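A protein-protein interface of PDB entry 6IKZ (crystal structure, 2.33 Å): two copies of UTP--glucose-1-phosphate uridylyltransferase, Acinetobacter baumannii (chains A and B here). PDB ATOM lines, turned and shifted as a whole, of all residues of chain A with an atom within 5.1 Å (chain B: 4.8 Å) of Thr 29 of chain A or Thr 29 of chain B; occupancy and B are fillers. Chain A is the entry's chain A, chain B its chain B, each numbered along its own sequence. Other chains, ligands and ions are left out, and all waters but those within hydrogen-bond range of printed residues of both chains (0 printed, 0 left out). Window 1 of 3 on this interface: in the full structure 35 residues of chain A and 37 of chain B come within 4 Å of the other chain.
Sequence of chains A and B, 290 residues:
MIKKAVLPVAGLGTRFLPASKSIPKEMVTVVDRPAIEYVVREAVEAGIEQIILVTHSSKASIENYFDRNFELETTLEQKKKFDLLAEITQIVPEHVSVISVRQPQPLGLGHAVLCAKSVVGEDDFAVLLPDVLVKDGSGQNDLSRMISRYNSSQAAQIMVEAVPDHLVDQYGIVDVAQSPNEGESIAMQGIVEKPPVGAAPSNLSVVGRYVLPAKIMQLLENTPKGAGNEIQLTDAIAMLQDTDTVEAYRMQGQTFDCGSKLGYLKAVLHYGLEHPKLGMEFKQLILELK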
ATOM      1  N   ALA A  19      29.732 -13.075  23.126  1.00  0.00           N
ATOM      2  CA  ALA A  19      28.918 -12.248  22.213  1.00  0.00           C
ATOM      3  C   ALA A  19      29.814 -11.511  21.213  1.00  0.00           C
ATOM      4  O   ALA A  19      29.381 -11.365  20.064  1.00  0.00           O
ATOM      5  CB  ALA A  19      28.078 -11.283  23.020  1.00  0.00           C
ATOM      6  N   ILE A  23      32.163 -10.788  16.333  1.00  0.00           N
ATOM      7  CA  ILE A  23      31.577  -9.521  15.796  1.00  0.00           C
ATOM      8  C   ILE A  23      31.970  -8.415  16.757  1.00  0.00           C
ATOM      9  O   ILE A  23      32.085  -8.652  17.941  1.00  0.00           O
ATOM     10  CB  ILE A  23      30.030  -9.570  15.664  1.00  0.00           C
ATOM     11  CG1 ILE A  23      29.353  -9.540  17.031  1.00  0.00           C
ATOM     12  CG2 ILE A  23      29.581 -10.773  14.873  1.00  0.00           C
ATOM     13  CD1 ILE A  23      27.847  -9.586  16.986  1.00  0.00           C
ATOM     14  N   MET A  27      28.491  -3.855  17.608  1.00  0.00           N
ATOM     15  CA  MET A  27      27.472  -4.365  16.661  1.00  0.00           C
ATOM     16  C   MET A  27      26.511  -5.292  17.399  1.00  0.00           C
ATOM     17  O   MET A  27      25.700  -5.922  16.752  1.00  0.00           O
ATOM     18  CB  MET A  27      28.117  -5.097  15.479  1.00  0.00           C
ATOM     19  CG  MET A  27      28.928  -4.161  14.578  1.00  0.00           C
ATOM     20  SD  MET A  27      27.888  -2.860  13.909  1.00  0.00           S
ATOM     21  CE  MET A  27      27.005  -3.820  12.686  1.00  0.00           C
ATOM     22  N   VAL A  28      26.565  -5.315  18.714  1.00  0.00           N
ATOM     23  CA  VAL A  28      25.617  -6.104  19.548  1.00  0.00           C
ATOM     24  C   VAL A  28      24.204  -5.533  19.377  1.00  0.00           C
ATOM     25  O   VAL A  28      24.035  -4.303  19.483  1.00  0.00           O
ATOM     26  CB  VAL A  28      26.076  -6.093  21.018  1.00  0.00           C
ATOM     27  CG2 VAL A  28      27.338  -6.922  21.125  1.00  0.00           C
ATOM     28  N   THR A  29      23.227  -6.407  19.178  1.00  0.00           N
ATOM     29  CA  THR A  29      21.807  -6.045  18.957  1.00  0.00           C
ATOM     30  C   THR A  29      21.280  -5.470  20.278  1.00  0.00           C
ATOM     31  O   THR A  29      21.274  -6.185  21.266  1.00  0.00           O
ATOM     32  CB  THR A  29      21.001  -7.225  18.387  1.00  0.00           C
ATOM     33  OG1 THR A  29      21.881  -8.001  17.564  1.00  0.00           O
ATOM     34  N   VAL A  30      20.911  -4.194  20.285  1.00  0.00           N
ATOM     35  CA  VAL A  30      20.085  -3.592  21.356  1.00  0.00           C
ATOM     36  C   VAL A  30      18.670  -3.446  20.797  1.00  0.00           C
ATOM     37  O   VAL A  30      18.411  -2.435  20.106  1.00  0.00           O
ATOM     38  CB  VAL A  30      20.685  -2.248  21.789  1.00  0.00           C
ATOM     39  CG1 VAL A  30      19.867  -1.598  22.895  1.00  0.00           C
ATOM     40  CG2 VAL A  30      22.141  -2.390  22.188  1.00  0.00           C
ATOM     41  N   VAL A  31      17.810  -4.433  21.063  1.00  0.00           N
ATOM     42  CA  VAL A  31      16.399  -4.517  20.566  1.00  0.00           C
ATOM     43  C   VAL A  31      16.395  -4.994  19.104  1.00  0.00           C
ATOM     44  O   VAL A  31      15.972  -6.137  18.837  1.00  0.00           O
ATOM     45  CB  VAL A  31      15.625  -3.191  20.707  1.00  0.00           C
ATOM     46  CG1 VAL A  31      14.126  -3.407  20.611  1.00  0.00           C
ATOM     47  CG2 VAL A  31      15.932  -2.463  21.997  1.00  0.00           C
ATOM     48  N   ARG A  33      18.711  -3.058  16.497  1.00  0.00           N
ATOM     49  CA  ARG A  33      19.882  -2.484  15.781  1.00  0.00           C
ATOM     50  C   ARG A  33      21.146  -2.606  16.616  1.00  0.00           C
ATOM     51  O   ARG A  33      21.087  -2.684  17.828  1.00  0.00           O
ATOM     52  CB  ARG A  33      19.653  -0.998  15.496  1.00  0.00           C
ATOM     53  CG  ARG A  33      19.242  -0.191  16.717  1.00  0.00           C
ATOM     54  CD  ARG A  33      17.807   0.299  16.620  1.00  0.00           C
ATOM     55  NE  ARG A  33      17.710   1.319  15.591  1.00  0.00           N
ATOM     56  CZ  ARG A  33      16.823   1.349  14.606  1.00  0.00           C
ATOM     57  NH1 ARG A  33      16.911   2.319  13.717  1.00  0.00           N
ATOM     58  NH2 ARG A  33      15.868   0.437  14.499  1.00  0.00           N
ATOM     59  N   PRO A  34      22.343  -2.550  16.012  1.00  0.00           N
ATOM     60  CA  PRO A  34      23.577  -2.497  16.785  1.00  0.00           C
ATOM     61  C   PRO A  34      23.665  -1.230  17.655  1.00  0.00           C
ATOM     62  O   PRO A  34      23.168  -0.178  17.260  1.00  0.00           O
ATOM     63  CB  PRO A  34      24.662  -2.527  15.691  1.00  0.00           C
ATOM     64  CG  PRO A  34      23.995  -1.890  14.537  1.00  0.00           C
ATOM     65  CD  PRO A  34      22.607  -2.511  14.572  1.00  0.00           C
ATOM     66  N   TYR A 264      24.110  -3.975  29.323  1.00  0.00           N
ATOM     67  CA  TYR A 264      23.438  -4.372  28.056  1.00  0.00           C
ATOM     68  C   TYR A 264      21.963  -4.756  28.300  1.00  0.00           C
ATOM     69  O   TYR A 264      21.083  -4.215  27.630  1.00  0.00           O
ATOM     70  CB  TYR A 264      24.239  -5.491  27.400  1.00  0.00           C
ATOM     71  CG  TYR A 264      23.558  -6.170  26.246  1.00  0.00           C
ATOM     72  CD1 TYR A 264      23.544  -5.610  24.976  1.00  0.00           C
ATOM     73  CD2 TYR A 264      22.959  -7.401  26.423  1.00  0.00           C
ATOM     74  CE1 TYR A 264      22.905  -6.234  23.915  1.00  0.00           C
ATOM     75  CE2 TYR A 264      22.355  -8.053  25.363  1.00  0.00           C
ATOM     76  CZ  TYR A 264      22.306  -7.462  24.113  1.00  0.00           C
ATOM     77  OH  TYR A 264      21.679  -8.140  23.107  1.00  0.00           O
ATOM     78  N   VAL A 268      18.621  -3.027  26.598  1.00  0.00           N
ATOM     79  CA  VAL A 268      17.594  -3.792  25.835  1.00  0.00           C
ATOM     80  C   VAL A 268      16.223  -3.521  26.471  1.00  0.00           C
ATOM     81  O   VAL A 268      15.345  -3.056  25.774  1.00  0.00           O
ATOM     82  CB  VAL A 268      17.917  -5.287  25.821  1.00  0.00           C
ATOM     83  CG1 VAL A 268      16.759  -6.084  25.251  1.00  0.00           C
ATOM     84  CG2 VAL A 268      19.219  -5.582  25.073  1.00  0.00           C
ATOM     85  N   ALA B  19      19.254  -5.103  12.273  1.00  0.00           N
ATOM     86  CA  ALA B  19      20.139  -5.880  13.177  1.00  0.00           C
ATOM     87  C   ALA B  19      21.154  -6.682  12.346  1.00  0.00           C
ATOM     88  O   ALA B  19      22.353  -6.722  12.701  1.00  0.00           O
ATOM     89  CB  ALA B  19      19.307  -6.782  14.066  1.00  0.00           C
ATOM     90  N   ILE B  23      25.978  -7.900   9.899  1.00  0.00           N
ATOM     91  CA  ILE B  23      26.334  -9.200  10.539  1.00  0.00           C
ATOM     92  C   ILE B  23      25.282 -10.240  10.190  1.00  0.00           C
ATOM     93  O   ILE B  23      24.112  -9.919   9.975  1.00  0.00           O
ATOM     94  CB  ILE B  23      26.457  -9.064  12.070  1.00  0.00           C
ATOM     95  CG1 ILE B  23      25.080  -8.871  12.713  1.00  0.00           C
ATOM     96  CG2 ILE B  23      27.468  -7.973  12.419  1.00  0.00           C
ATOM     97  CD1 ILE B  23      25.138  -8.424  14.127  1.00  0.00           C
ATOM     98  N   MET B  27      24.345 -14.446  14.115  1.00  0.00           N
ATOM     99  CA  MET B  27      25.364 -13.910  15.053  1.00  0.00           C
ATOM    100  C   MET B  27      24.739 -12.808  15.919  1.00  0.00           C
ATOM    101  O   MET B  27      25.450 -12.193  16.730  1.00  0.00           O
ATOM    102  CB  MET B  27      26.541 -13.345  14.255  1.00  0.00           C
ATOM    103  CG  MET B  27      27.291 -14.415  13.518  1.00  0.00           C
ATOM    104  SD  MET B  27      27.915 -15.617  14.690  1.00  0.00           S
ATOM    105  CE  MET B  27      28.994 -14.526  15.609  1.00  0.00           C
ATOM    106  N   VAL B  28      23.444 -12.585  15.783  1.00  0.00           N
ATOM    107  CA  VAL B  28      22.689 -11.620  16.630  1.00  0.00           C
ATOM    108  C   VAL B  28      22.698 -12.166  18.053  1.00  0.00           C
ATOM    109  O   VAL B  28      22.602 -13.405  18.213  1.00  0.00           O
ATOM    110  CB  VAL B  28      21.266 -11.420  16.081  1.00  0.00           C
ATOM    111  CG1 VAL B  28      20.210 -11.268  17.163  1.00  0.00           C
ATOM    112  CG2 VAL B  28      21.234 -10.245  15.115  1.00  0.00           C
ATOM    113  N   THR B  29      22.802 -11.274  19.042  1.00  0.00           N
ATOM    114  CA  THR B  29      23.177 -11.640  20.420  1.00  0.00           C
ATOM    115  C   THR B  29      21.871 -11.888  21.164  1.00  0.00           C
ATOM    116  O   THR B  29      21.001 -11.039  21.107  1.00  0.00           O
ATOM    117  CB  THR B  29      24.227 -10.672  20.997  1.00  0.00           C
ATOM    118  OG1 THR B  29      23.698  -9.366  21.161  1.00  0.00           O
ATOM    119  CG2 THR B  29      25.457 -10.561  20.116  1.00  0.00           C
ATOM    120  N   VAL B  30      21.761 -13.091  21.733  1.00  0.00           N
ATOM    121  CA  VAL B  30      20.679 -13.567  22.627  1.00  0.00           C
ATOM    122  C   VAL B  30      21.287 -13.686  24.029  1.00  0.00           C
ATOM    123  O   VAL B  30      21.917 -14.710  24.340  1.00  0.00           O
ATOM    124  CB  VAL B  30      20.096 -14.895  22.112  1.00  0.00           C
ATOM    125  CG1 VAL B  30      18.934 -15.392  22.965  1.00  0.00           C
ATOM    126  CG2 VAL B  30      19.673 -14.772  20.653  1.00  0.00           C
ATOM    127  N   VAL B  31      21.146 -12.613  24.802  1.00  0.00           N
ATOM    128  CA  VAL B  31      21.611 -12.454  26.201  1.00  0.00           C
ATOM    129  C   VAL B  31      23.094 -12.103  26.172  1.00  0.00           C
ATOM    130  O   VAL B  31      23.399 -10.936  26.505  1.00  0.00           O
ATOM    131  CB  VAL B  31      21.287 -13.688  27.060  1.00  0.00           C
ATOM    132  CG1 VAL B  31      21.645 -13.455  28.515  1.00  0.00           C
ATOM    133  CG2 VAL B  31      19.808 -14.054  26.968  1.00  0.00           C
ATOM    134  N   ARG B  33      25.542 -14.130  23.813  1.00  0.00           N
ATOM    135  CA  ARG B  33      26.157 -15.051  22.834  1.00  0.00           C
ATOM    136  C   ARG B  33      25.272 -15.039  21.593  1.00  0.00           C
ATOM    137  O   ARG B  33      24.086 -14.696  21.659  1.00  0.00           O
ATOM    138  CB  ARG B  33      26.360 -16.448  23.450  1.00  0.00           C
ATOM    139  CG  ARG B  33      25.083 -17.173  23.857  1.00  0.00           C
ATOM    140  CD  ARG B  33      25.144 -17.852  25.220  1.00  0.00           C
ATOM    141  NE  ARG B  33      26.410 -18.552  25.381  1.00  0.00           N
ATOM    142  CZ  ARG B  33      27.248 -18.427  26.401  1.00  0.00           C
ATOM    143  NH1 ARG B  33      28.378 -19.110  26.385  1.00  0.00           N
ATOM    144  NH2 ARG B  33      26.969 -17.634  27.422  1.00  0.00           N
ATOM    145  N   PRO B  34      25.851 -15.376  20.428  1.00  0.00           N
ATOM    146  CA  PRO B  34      25.107 -15.417  19.185  1.00  0.00           C
ATOM    147  C   PRO B  34      24.064 -16.526  19.245  1.00  0.00           C
ATOM    148  O   PRO B  34      24.295 -17.491  19.960  1.00  0.00           O
ATOM    149  CB  PRO B  34      26.160 -15.737  18.127  1.00  0.00           C
ATOM    150  CG  PRO B  34      27.286 -16.379  18.889  1.00  0.00           C
ATOM    151  CD  PRO B  34      27.265 -15.719  20.244  1.00  0.00           C
ATOM    152  N   TYR B 264      12.442 -12.769  18.771  1.00  0.00           N
ATOM    153  CA  TYR B 264      13.827 -12.564  19.282  1.00  0.00           C
ATOM    154  C   TYR B 264      13.732 -11.888  20.661  1.00  0.00           C
ATOM    155  O   TYR B 264      14.377 -12.352  21.625  1.00  0.00           O
ATOM    156  CB  TYR B 264      14.718 -11.848  18.257  1.00  0.00           C
ATOM    157  CG  TYR B 264      15.881 -11.107  18.862  1.00  0.00           C
ATOM    158  CD1 TYR B 264      15.699  -9.844  19.384  1.00  0.00           C
ATOM    159  CD2 TYR B 264      17.146 -11.669  18.961  1.00  0.00           C
ATOM    160  CE1 TYR B 264      16.738  -9.147  19.972  1.00  0.00           C
ATOM    161  CE2 TYR B 264      18.198 -10.989  19.571  1.00  0.00           C
ATOM    162  CZ  TYR B 264      18.001  -9.708  20.069  1.00  0.00           C
ATOM    163  OH  TYR B 264      18.987  -8.973  20.695  1.00  0.00           O
ATOM    164  N   VAL B 268      15.307 -13.526  24.300  1.00  0.00           N
ATOM    165  CA  VAL B 268      16.166 -12.749  25.236  1.00  0.00           C
ATOM    166  C   VAL B 268      15.555 -12.810  26.635  1.00  0.00           C
ATOM    167  O   VAL B 268      16.283 -13.190  27.568  1.00  0.00           O
ATOM    168  CB  VAL B 268      16.308 -11.291  24.756  1.00  0.00           C
ATOM    169  CG1 VAL B 268      16.951 -10.398  25.815  1.00  0.00           C
ATOM    170  CG2 VAL B 268      17.061 -11.230  23.433  1.00  0.00           C
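Of the 11 printed residues of chain A, 6 touch a printed residue of chain B.
Printed residues of chain A that touch a printed residue of chain B: Ala 19, Ile 23, Met 27, Thr 29, Val 31 and Tyr 264.
Hydrophobic or aromatic side chains of chain A that line the printed part of chain B: Ala 19, Ile 23 and Tyr 264.
Among the printed residues, 11 pairs touch across the chains.
Among the printed residues, no Asp or Glu carboxylate lies within 4 Å of a Lys or Arg side-chain nitrogen of the other chain.
Ala 19 of chain A touches Arg 33 of chain B, but with the chains exchanged Arg 33 of chain A does not touch Ala 19 of chain B (4.3 Å).
Thr 29 of chain B touches its own counterpart, Thr 29 of chain A.
Thr 29 of chain A touches Tyr 264 of chain B, and with the chains exchanged Tyr 264 of chain A touches Thr 29 of chain B.
Val 31 of chain A touches Tyr 264 of chain B, and with the chains exchanged Tyr 264 of chain A touches Val 31 of chain B.
11 positions are printed for both chains.
Of the 11 pairs that touch across the chains among the printed residues, 8 have their exchanged pair printed and touching as well.
Of the printed residues of chain B, Tyr 264 of chain A touches Thr 29 (3.1 Å), Val 31 (3.3 Å) and Tyr 264 (3.7 Å).
Printed residues of chain A within 4 Å of Val 28 of chain B: Thr 29.
Pro 34 of chain A touches none of the printed residues of chain B.
Arg 33 of chain A touches none of the printed residues of chain B.
The nearest residue of chain B that does not touch Thr 29 of chain A is Ala 19 of chain B (4.5 Å).
The nearest printed residue of chain B that does not touch Ala 19 of chain A is Pro 34 of chain B (4.3 Å).
The side-chain hydroxyl of Tyr 264 of chain A lies within hydrogen-bond range of the side-chain hydroxyl of Thr 29 of chain B (3.1 Å).
Ala 19 of chain A touches Thr 29 of chain B.
CB of Ala 19 of chain A touches N of Arg 33 of chain B, 3.9 Å away.
Ile 23 of chain A touches Met 27 of chain B.
Ile 23 of chain B touches Met 27 of chain A (CD1 to O, 3.7 Å).
Val 28 of chain B touches Thr 29 of chain A (CG2 to OG1, 3.4 Å).
Thr 29 of chain A touches Thr 29 of chain B.
Thr 29 of chain A touches Tyr 264 of chain B (CB to OH, 3.5 Å).
Val 31 of chain A touches Tyr 264 of chain B.
Val 31 of chain B touches Tyr 264 of chain A.
OH of Tyr 264 of chain A touches OH of Tyr 264 of chain B, at 3.7 Å.
The side-chain hydroxyl (OH) of Tyr 264 of chain A sits at hydrogen-bond distance from the backbone carbonyl oxygen (O) of Thr 29 of chain A, 2.7 Å away.
The backbone carbonyl oxygen (O) of Thr 29 of chain B sits at hydrogen-bond distance from the side-chain hydroxyl (OH) of Tyr 264 of chain B, 2.9 Å away.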
